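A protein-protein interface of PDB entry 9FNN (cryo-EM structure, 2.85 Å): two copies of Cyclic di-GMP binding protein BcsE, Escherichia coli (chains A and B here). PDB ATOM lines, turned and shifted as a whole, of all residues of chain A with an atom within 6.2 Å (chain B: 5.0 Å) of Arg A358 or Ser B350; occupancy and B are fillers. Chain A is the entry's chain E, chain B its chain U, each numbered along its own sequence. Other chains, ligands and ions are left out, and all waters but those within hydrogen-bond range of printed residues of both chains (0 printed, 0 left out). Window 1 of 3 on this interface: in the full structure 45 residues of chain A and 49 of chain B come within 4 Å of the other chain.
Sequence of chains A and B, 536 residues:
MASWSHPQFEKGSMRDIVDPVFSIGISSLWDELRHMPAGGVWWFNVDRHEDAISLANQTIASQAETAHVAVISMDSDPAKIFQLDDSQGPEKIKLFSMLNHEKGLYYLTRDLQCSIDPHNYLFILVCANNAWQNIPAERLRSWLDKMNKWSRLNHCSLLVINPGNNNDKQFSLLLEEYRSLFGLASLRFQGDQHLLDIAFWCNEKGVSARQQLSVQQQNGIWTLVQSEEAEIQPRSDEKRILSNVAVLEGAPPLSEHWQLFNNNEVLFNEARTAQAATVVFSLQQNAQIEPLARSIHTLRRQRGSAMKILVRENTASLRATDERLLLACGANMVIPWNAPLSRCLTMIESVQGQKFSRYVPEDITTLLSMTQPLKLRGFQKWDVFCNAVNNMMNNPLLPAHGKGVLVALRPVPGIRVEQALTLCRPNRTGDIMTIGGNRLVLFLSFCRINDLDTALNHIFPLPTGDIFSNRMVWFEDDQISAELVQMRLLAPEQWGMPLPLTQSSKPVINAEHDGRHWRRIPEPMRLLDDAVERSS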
ATOM      1  N   ARG A 300      -3.556   6.155  24.945  1.00  0.00           N
ATOM      2  CA  ARG A 300      -3.286   5.264  26.064  1.00  0.00           C
ATOM      3  C   ARG A 300      -1.859   4.738  26.046  1.00  0.00           C
ATOM      4  O   ARG A 300      -1.348   4.334  27.096  1.00  0.00           O
ATOM      5  CB  ARG A 300      -4.277   4.101  26.059  1.00  0.00           C
ATOM      6  CG  ARG A 300      -4.221   3.232  27.299  1.00  0.00           C
ATOM      7  CD  ARG A 300      -4.521   4.039  28.542  1.00  0.00           C
ATOM      8  NE  ARG A 300      -5.928   4.406  28.626  1.00  0.00           N
ATOM      9  CZ  ARG A 300      -6.443   5.179  29.570  1.00  0.00           C
ATOM     10  NH1 ARG A 300      -5.689   5.699  30.525  1.00  0.00           N
ATOM     11  NH2 ARG A 300      -7.745   5.435  29.558  1.00  0.00           N
ATOM     12  N   GLU A 323     -17.464  -1.752  20.462  1.00  0.00           N
ATOM     13  CA  GLU A 323     -17.269  -1.300  21.833  1.00  0.00           C
ATOM     14  C   GLU A 323     -16.151  -2.079  22.509  1.00  0.00           C
ATOM     15  O   GLU A 323     -15.346  -1.502  23.249  1.00  0.00           O
ATOM     16  CB  GLU A 323     -18.572  -1.425  22.618  1.00  0.00           C
ATOM     17  CG  GLU A 323     -18.560  -0.701  23.948  1.00  0.00           C
ATOM     18  CD  GLU A 323     -19.950  -0.517  24.521  1.00  0.00           C
ATOM     19  OE1 GLU A 323     -20.929  -0.902  23.847  1.00  0.00           O
ATOM     20  OE2 GLU A 323     -20.066   0.012  25.647  1.00  0.00           O
ATOM     21  N   LEU A 326     -12.922  -0.622  21.215  1.00  0.00           N
ATOM     22  CA  LEU A 326     -12.604   0.663  21.827  1.00  0.00           C
ATOM     23  C   LEU A 326     -12.124   0.484  23.261  1.00  0.00           C
ATOM     24  O   LEU A 326     -11.196   1.170  23.702  1.00  0.00           O
ATOM     25  CB  LEU A 326     -13.817   1.588  21.770  1.00  0.00           C
ATOM     26  CG  LEU A 326     -14.192   2.099  20.379  1.00  0.00           C
ATOM     27  CD1 LEU A 326     -15.507   2.842  20.411  1.00  0.00           C
ATOM     28  CD2 LEU A 326     -13.095   2.988  19.836  1.00  0.00           C
ATOM     29  N   LEU A 327     -12.742  -0.434  24.005  1.00  0.00           N
ATOM     30  CA  LEU A 327     -12.286  -0.713  25.361  1.00  0.00           C
ATOM     31  C   LEU A 327     -10.883  -1.299  25.361  1.00  0.00           C
ATOM     32  O   LEU A 327     -10.056  -0.953  26.212  1.00  0.00           O
ATOM     33  CB  LEU A 327     -13.261  -1.659  26.059  1.00  0.00           C
ATOM     34  CG  LEU A 327     -14.650  -1.101  26.354  1.00  0.00           C
ATOM     35  CD1 LEU A 327     -15.594  -2.219  26.737  1.00  0.00           C
ATOM     36  CD2 LEU A 327     -14.578  -0.062  27.450  1.00  0.00           C
ATOM     37  N   ALA A 328     -10.597  -2.197  24.417  1.00  0.00           N
ATOM     38  CA  ALA A 328      -9.271  -2.796  24.334  1.00  0.00           C
ATOM     39  C   ALA A 328      -8.214  -1.758  23.989  1.00  0.00           C
ATOM     40  O   ALA A 328      -7.098  -1.802  24.518  1.00  0.00           O
ATOM     41  CB  ALA A 328      -9.270  -3.925  23.305  1.00  0.00           C
ATOM     42  N   CYS A 329      -8.543  -0.818  23.102  1.00  0.00           N
ATOM     43  CA  CYS A 329      -7.575   0.192  22.695  1.00  0.00           C
ATOM     44  C   CYS A 329      -7.215   1.150  23.822  1.00  0.00           C
ATOM     45  O   CYS A 329      -6.193   1.838  23.724  1.00  0.00           O
ATOM     46  CB  CYS A 329      -8.104   0.973  21.495  1.00  0.00           C
ATOM     47  SG  CYS A 329      -8.213   0.006  19.976  1.00  0.00           S
ATOM     48  N   GLY A 330      -8.013   1.214  24.883  1.00  0.00           N
ATOM     49  CA  GLY A 330      -7.657   2.041  26.018  1.00  0.00           C
ATOM     50  C   GLY A 330      -8.743   2.961  26.537  1.00  0.00           C
ATOM     51  O   GLY A 330      -8.459   3.856  27.337  1.00  0.00           O
ATOM     52  N   ALA A 331      -9.983   2.762  26.104  1.00  0.00           N
ATOM     53  CA  ALA A 331     -11.084   3.583  26.587  1.00  0.00           C
ATOM     54  C   ALA A 331     -11.584   3.052  27.923  1.00  0.00           C
ATOM     55  O   ALA A 331     -11.766   1.844  28.090  1.00  0.00           O
ATOM     56  CB  ALA A 331     -12.221   3.610  25.569  1.00  0.00           C
ATOM     57  N   ASN A 332     -11.798   3.959  28.878  1.00  0.00           N
ATOM     58  CA  ASN A 332     -12.294   3.547  30.188  1.00  0.00           C
ATOM     59  C   ASN A 332     -13.678   2.920  30.078  1.00  0.00           C
ATOM     60  O   ASN A 332     -13.909   1.813  30.575  1.00  0.00           O
ATOM     61  CB  ASN A 332     -12.313   4.737  31.144  1.00  0.00           C
ATOM     62  CG  ASN A 332     -10.966   4.998  31.770  1.00  0.00           C
ATOM     63  OD1 ASN A 332     -10.086   5.587  31.149  1.00  0.00           O
ATOM     64  ND2 ASN A 332     -10.800   4.569  33.013  1.00  0.00           N
ATOM     65  N   MET A 333     -14.613   3.614  29.434  1.00  0.00           N
ATOM     66  CA  MET A 333     -15.909   3.019  29.137  1.00  0.00           C
ATOM     67  C   MET A 333     -16.580   3.801  28.022  1.00  0.00           C
ATOM     68  O   MET A 333     -16.253   4.961  27.764  1.00  0.00           O
ATOM     69  CB  MET A 333     -16.814   2.971  30.371  1.00  0.00           C
ATOM     70  CG  MET A 333     -17.215   4.326  30.905  1.00  0.00           C
ATOM     71  SD  MET A 333     -18.515   4.188  32.136  1.00  0.00           S
ATOM     72  CE  MET A 333     -18.357   5.768  32.947  1.00  0.00           C
ATOM     73  N   VAL A 334     -17.529   3.141  27.368  1.00  0.00           N
ATOM     74  CA  VAL A 334     -18.317   3.722  26.291  1.00  0.00           C
ATOM     75  C   VAL A 334     -19.721   3.971  26.818  1.00  0.00           C
ATOM     76  O   VAL A 334     -20.371   3.051  27.328  1.00  0.00           O
ATOM     77  CB  VAL A 334     -18.343   2.805  25.056  1.00  0.00           C
ATOM     78  CG1 VAL A 334     -19.311   3.334  24.022  1.00  0.00           C
ATOM     79  CG2 VAL A 334     -16.953   2.681  24.465  1.00  0.00           C
ATOM     80  N   LYS A 355      -7.562   4.474  37.514  1.00  0.00           N
ATOM     81  CA  LYS A 355      -6.432   4.260  36.624  1.00  0.00           C
ATOM     82  C   LYS A 355      -6.709   3.068  35.721  1.00  0.00           C
ATOM     83  O   LYS A 355      -7.350   2.099  36.137  1.00  0.00           O
ATOM     84  CB  LYS A 355      -5.144   4.032  37.413  1.00  0.00           C
ATOM     85  CG  LYS A 355      -4.863   5.091  38.458  1.00  0.00           C
ATOM     86  CD  LYS A 355      -3.376   5.197  38.750  1.00  0.00           C
ATOM     87  CE  LYS A 355      -2.791   3.859  39.173  1.00  0.00           C
ATOM     88  NZ  LYS A 355      -3.405   3.355  40.432  1.00  0.00           N
ATOM     89  N   PHE A 356      -6.227   3.146  34.484  1.00  0.00           N
ATOM     90  CA  PHE A 356      -6.455   2.097  33.493  1.00  0.00           C
ATOM     91  C   PHE A 356      -5.405   1.013  33.676  1.00  0.00           C
ATOM     92  O   PHE A 356      -4.263   1.155  33.235  1.00  0.00           O
ATOM     93  CB  PHE A 356      -6.409   2.675  32.087  1.00  0.00           C
ATOM     94  CG  PHE A 356      -7.090   1.824  31.063  1.00  0.00           C
ATOM     95  CD1 PHE A 356      -8.463   1.835  30.945  1.00  0.00           C
ATOM     96  CD2 PHE A 356      -6.358   1.019  30.212  1.00  0.00           C
ATOM     97  CE1 PHE A 356      -9.095   1.057  30.004  1.00  0.00           C
ATOM     98  CE2 PHE A 356      -6.988   0.238  29.269  1.00  0.00           C
ATOM     99  CZ  PHE A 356      -8.356   0.260  29.166  1.00  0.00           C
ATOM    100  N   SER A 357      -5.791  -0.083  34.325  1.00  0.00           N
ATOM    101  CA  SER A 357      -4.877  -1.174  34.633  1.00  0.00           C
ATOM    102  C   SER A 357      -4.910  -2.298  33.607  1.00  0.00           C
ATOM    103  O   SER A 357      -4.118  -3.237  33.719  1.00  0.00           O
ATOM    104  CB  SER A 357      -5.189  -1.738  36.020  1.00  0.00           C
ATOM    105  OG  SER A 357      -5.155  -0.717  37.000  1.00  0.00           O
ATOM    106  N   ARG A 358      -5.796  -2.233  32.619  1.00  0.00           N
ATOM    107  CA  ARG A 358      -5.864  -3.277  31.609  1.00  0.00           C
ATOM    108  C   ARG A 358      -4.720  -3.125  30.613  1.00  0.00           C
ATOM    109  O   ARG A 358      -4.221  -2.023  30.371  1.00  0.00           O
ATOM    110  CB  ARG A 358      -7.207  -3.240  30.880  1.00  0.00           C
ATOM    111  CG  ARG A 358      -7.705  -4.609  30.458  1.00  0.00           C
ATOM    112  CD  ARG A 358      -8.943  -4.541  29.579  1.00  0.00           C
ATOM    113  NE  ARG A 358     -10.059  -3.864  30.228  1.00  0.00           N
ATOM    114  CZ  ARG A 358     -10.661  -2.787  29.746  1.00  0.00           C
ATOM    115  NH1 ARG A 358     -10.294  -2.246  28.597  1.00  0.00           N
ATOM    116  NH2 ARG A 358     -11.661  -2.242  30.432  1.00  0.00           N
ATOM    117  N   TYR A 359      -4.306  -4.250  30.033  1.00  0.00           N
ATOM    118  CA  TYR A 359      -3.175  -4.257  29.115  1.00  0.00           C
ATOM    119  C   TYR A 359      -3.621  -3.879  27.711  1.00  0.00           C
ATOM    120  O   TYR A 359      -4.577  -4.448  27.178  1.00  0.00           O
ATOM    121  CB  TYR A 359      -2.504  -5.630  29.095  1.00  0.00           C
ATOM    122  CG  TYR A 359      -1.546  -5.807  27.936  1.00  0.00           C
ATOM    123  CD1 TYR A 359      -0.298  -5.202  27.942  1.00  0.00           C
ATOM    124  CD2 TYR A 359      -1.895  -6.577  26.834  1.00  0.00           C
ATOM    125  CE1 TYR A 359       0.577  -5.356  26.884  1.00  0.00           C
ATOM    126  CE2 TYR A 359      -1.024  -6.737  25.773  1.00  0.00           C
ATOM    127  CZ  TYR A 359       0.209  -6.125  25.803  1.00  0.00           C
ATOM    128  OH  TYR A 359       1.076  -6.284  24.748  1.00  0.00           O
ATOM    129  N   VAL A 360      -2.923  -2.925  27.113  1.00  0.00           N
ATOM    130  CA  VAL A 360      -3.184  -2.471  25.751  1.00  0.00           C
ATOM    131  C   VAL A 360      -2.036  -2.956  24.871  1.00  0.00           C
ATOM    132  O   VAL A 360      -0.890  -2.532  25.072  1.00  0.00           O
ATOM    133  CB  VAL A 360      -3.328  -0.944  25.678  1.00  0.00           C
ATOM    134  CG1 VAL A 360      -3.790  -0.527  24.294  1.00  0.00           C
ATOM    135  CG2 VAL A 360      -4.298  -0.455  26.738  1.00  0.00           C
ATOM    136  N   MET B 333     -19.428   1.480  39.032  1.00  0.00           N
ATOM    137  CA  MET B 333     -20.261   2.072  38.000  1.00  0.00           C
ATOM    138  C   MET B 333     -21.718   1.766  38.298  1.00  0.00           C
ATOM    139  O   MET B 333     -22.048   0.667  38.747  1.00  0.00           O
ATOM    140  CB  MET B 333     -19.868   1.544  36.616  1.00  0.00           C
ATOM    141  CG  MET B 333     -20.862   1.832  35.515  1.00  0.00           C
ATOM    142  SD  MET B 333     -20.176   1.478  33.892  1.00  0.00           S
ATOM    143  CE  MET B 333     -19.451  -0.128  34.181  1.00  0.00           C
ATOM    144  N   THR B 346     -22.116  -5.251  28.136  1.00  0.00           N
ATOM    145  CA  THR B 346     -20.866  -4.684  27.640  1.00  0.00           C
ATOM    146  C   THR B 346     -20.227  -3.769  28.680  1.00  0.00           C
ATOM    147  O   THR B 346     -19.004  -3.768  28.852  1.00  0.00           O
ATOM    148  CB  THR B 346     -21.104  -3.936  26.331  1.00  0.00           C
ATOM    149  OG1 THR B 346     -22.002  -4.690  25.510  1.00  0.00           O
ATOM    150  CG2 THR B 346     -19.796  -3.767  25.588  1.00  0.00           C
ATOM    151  N   MET B 347     -21.038  -2.992  29.398  1.00  0.00           N
ATOM    152  CA  MET B 347     -20.495  -2.171  30.473  1.00  0.00           C
ATOM    153  C   MET B 347     -19.951  -3.026  31.609  1.00  0.00           C
ATOM    154  O   MET B 347     -18.955  -2.654  32.240  1.00  0.00           O
ATOM    155  CB  MET B 347     -21.560  -1.203  30.986  1.00  0.00           C
ATOM    156  CG  MET B 347     -21.742   0.018  30.097  1.00  0.00           C
ATOM    157  SD  MET B 347     -22.997   1.174  30.672  1.00  0.00           S
ATOM    158  CE  MET B 347     -24.487   0.343  30.140  1.00  0.00           C
ATOM    159  N   ILE B 348     -20.587  -4.164  31.883  1.00  0.00           N
ATOM    160  CA  ILE B 348     -20.070  -5.086  32.890  1.00  0.00           C
ATOM    161  C   ILE B 348     -18.684  -5.568  32.494  1.00  0.00           C
ATOM    162  O   ILE B 348     -17.756  -5.595  33.310  1.00  0.00           O
ATOM    163  CB  ILE B 348     -21.037  -6.267  33.088  1.00  0.00           C
ATOM    164  CG1 ILE B 348     -22.262  -5.835  33.891  1.00  0.00           C
ATOM    165  CG2 ILE B 348     -20.335  -7.424  33.764  1.00  0.00           C
ATOM    166  CD1 ILE B 348     -23.244  -6.951  34.148  1.00  0.00           C
ATOM    167  N   GLU B 349     -18.521  -5.947  31.227  1.00  0.00           N
ATOM    168  CA  GLU B 349     -17.218  -6.428  30.783  1.00  0.00           C
ATOM    169  C   GLU B 349     -16.207  -5.299  30.619  1.00  0.00           C
ATOM    170  O   GLU B 349     -15.008  -5.570  30.527  1.00  0.00           O
ATOM    171  CB  GLU B 349     -17.355  -7.208  29.477  1.00  0.00           C
ATOM    172  CG  GLU B 349     -17.397  -6.359  28.232  1.00  0.00           C
ATOM    173  CD  GLU B 349     -17.814  -7.150  27.010  1.00  0.00           C
ATOM    174  OE1 GLU B 349     -18.068  -8.366  27.144  1.00  0.00           O
ATOM    175  OE2 GLU B 349     -17.893  -6.556  25.915  1.00  0.00           O
ATOM    176  N   SER B 350     -16.662  -4.047  30.580  1.00  0.00           N
ATOM    177  CA  SER B 350     -15.739  -2.925  30.442  1.00  0.00           C
ATOM    178  C   SER B 350     -14.865  -2.713  31.670  1.00  0.00           C
ATOM    179  O   SER B 350     -13.785  -2.130  31.550  1.00  0.00           O
ATOM    180  CB  SER B 350     -16.511  -1.639  30.156  1.00  0.00           C
ATOM    181  OG  SER B 350     -17.189  -1.187  31.315  1.00  0.00           O
ATOM    182  N   VAL B 351     -15.303  -3.165  32.849  1.00  0.00           N
ATOM    183  CA  VAL B 351     -14.607  -2.847  34.092  1.00  0.00           C
ATOM    184  C   VAL B 351     -13.616  -3.928  34.501  1.00  0.00           C
ATOM    185  O   VAL B 351     -12.983  -3.809  35.559  1.00  0.00           O
ATOM    186  CB  VAL B 351     -15.643  -2.589  35.206  1.00  0.00           C
ATOM    187  CG1 VAL B 351     -16.148  -3.895  35.790  1.00  0.00           C
ATOM    188  CG2 VAL B 351     -15.075  -1.673  36.285  1.00  0.00           C
ATOM    189  N   GLN B 352     -13.446  -4.968  33.692  1.00  0.00           N
ATOM    190  CA  GLN B 352     -12.586  -6.083  34.061  1.00  0.00           C
ATOM    191  C   GLN B 352     -11.132  -5.645  34.163  1.00  0.00           C
ATOM    192  O   GLN B 352     -10.660  -4.811  33.390  1.00  0.00           O
ATOM    193  CB  GLN B 352     -12.720  -7.208  33.043  1.00  0.00           C
ATOM    194  CG  GLN B 352     -14.138  -7.685  32.832  1.00  0.00           C
ATOM    195  CD  GLN B 352     -14.715  -8.348  34.056  1.00  0.00           C
ATOM    196  OE1 GLN B 352     -15.833  -8.048  34.467  1.00  0.00           O
ATOM    197  NE2 GLN B 352     -13.960  -9.266  34.643  1.00  0.00           N
ATOM    198  N   GLY B 353     -10.423  -6.214  35.133  1.00  0.00           N
ATOM    199  CA  GLY B 353      -9.017  -5.928  35.307  1.00  0.00           C
ATOM    200  C   GLY B 353      -8.705  -4.581  35.908  1.00  0.00           C
ATOM    201  O   GLY B 353      -7.537  -4.190  35.937  1.00  0.00           O
ATOM    202  N   GLN B 354      -9.709  -3.861  36.394  1.00  0.00           N
ATOM    203  CA  GLN B 354      -9.540  -2.507  36.893  1.00  0.00           C
ATOM    204  C   GLN B 354      -9.586  -2.505  38.412  1.00  0.00           C
ATOM    205  O   GLN B 354     -10.351  -3.259  39.020  1.00  0.00           O
ATOM    206  CB  GLN B 354     -10.621  -1.579  36.338  1.00  0.00           C
ATOM    207  CG  GLN B 354     -10.648  -1.494  34.825  1.00  0.00           C
ATOM    208  CD  GLN B 354      -9.447  -0.772  34.252  1.00  0.00           C
ATOM    209  OE1 GLN B 354      -8.672  -0.155  34.978  1.00  0.00           O
ATOM    210  NE2 GLN B 354      -9.291  -0.842  32.938  1.00  0.00           N
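Met B333 touches its own counterpart, Met A333. Of the 10 pairs that touch across the chains among the printed residues, 1 has its exchanged pair printed and touching as well.
Hydrophobic or aromatic side chains of chain B within 4 Å of the printed part of chain A: Met B333. Of the 17 printed residues of chain A, 7 touch a printed residue of chain B. Hydrophobic or aromatic side chains of chain A within 4 Å of the printed part of chain B: Leu A327, Met A333 and Phe A356. Among the printed residues, 10 pairs touch across the chains. Among the printed residues, no Asp or Glu carboxylate lies within 4 Å of a Lys or Arg side-chain nitrogen of the other chain.
Of the printed residues of chain B, Glu A323 touches Thr B346 (3.4 Å). Ala A328 touches none of the printed residues of chain B. Printed residues of chain B within 4 Å of Lys A355: Gln B354. Of the printed residues of chain B, Phe A356 touches Gln B354. Of the printed residues of chain B, Arg A358 touches Ser B350, Gln B352 and Gln B354. Ser B350 touches two residues of chain A. Of the printed residues of chain A, Gln B354 touches Lys A355, Phe A356, Ser A357 and Arg A358. The nearest residue of chain A that does not touch Ser B350 is Asn A332 (4.1 Å). The nearest printed residue of chain B that does not touch Met A333 is Ser B350 (4.3 Å).
OE1 of Gln B354 lies close to O of Lys A355, at 2.9 Å. The backbone NH (N) of Ser A357 is in hydrogen-bond range of the side-chain amide oxygen (OE1) of Gln B354 (3.0 Å). The backbone carbonyl oxygen of Ser B350 sits at hydrogen-bond distance from the guanidinium group of Arg A358, at 2.4 Å. The guanidinium group of Arg A358 sits at hydrogen-bond distance from the backbone carbonyl oxygen of Gln B352. SD of Met B333 sits close to SD of Met A333 (3.6 Å).
O of Leu A327 sits at hydrogen-bond distance from NH1 of Arg A358. O of Met B347 is in hydrogen-bond range of OG of Ser B350, 2.5 Å away. The backbone carbonyl oxygen of Ile B348 lies close to the side-chain amide oxygen of Gln B352 (3.3 Å).
CD of Glu A323 touches CG2 of Thr B346 (3.4 Å). Leu A327 touches Ser B350 (CD1 to CB, 3.6 Å). Phe A356 touches Gln B354. Ser A357 touches Gly B353. Gln B354 touches Arg A358 (NE2 to NH2, 3.7 Å).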
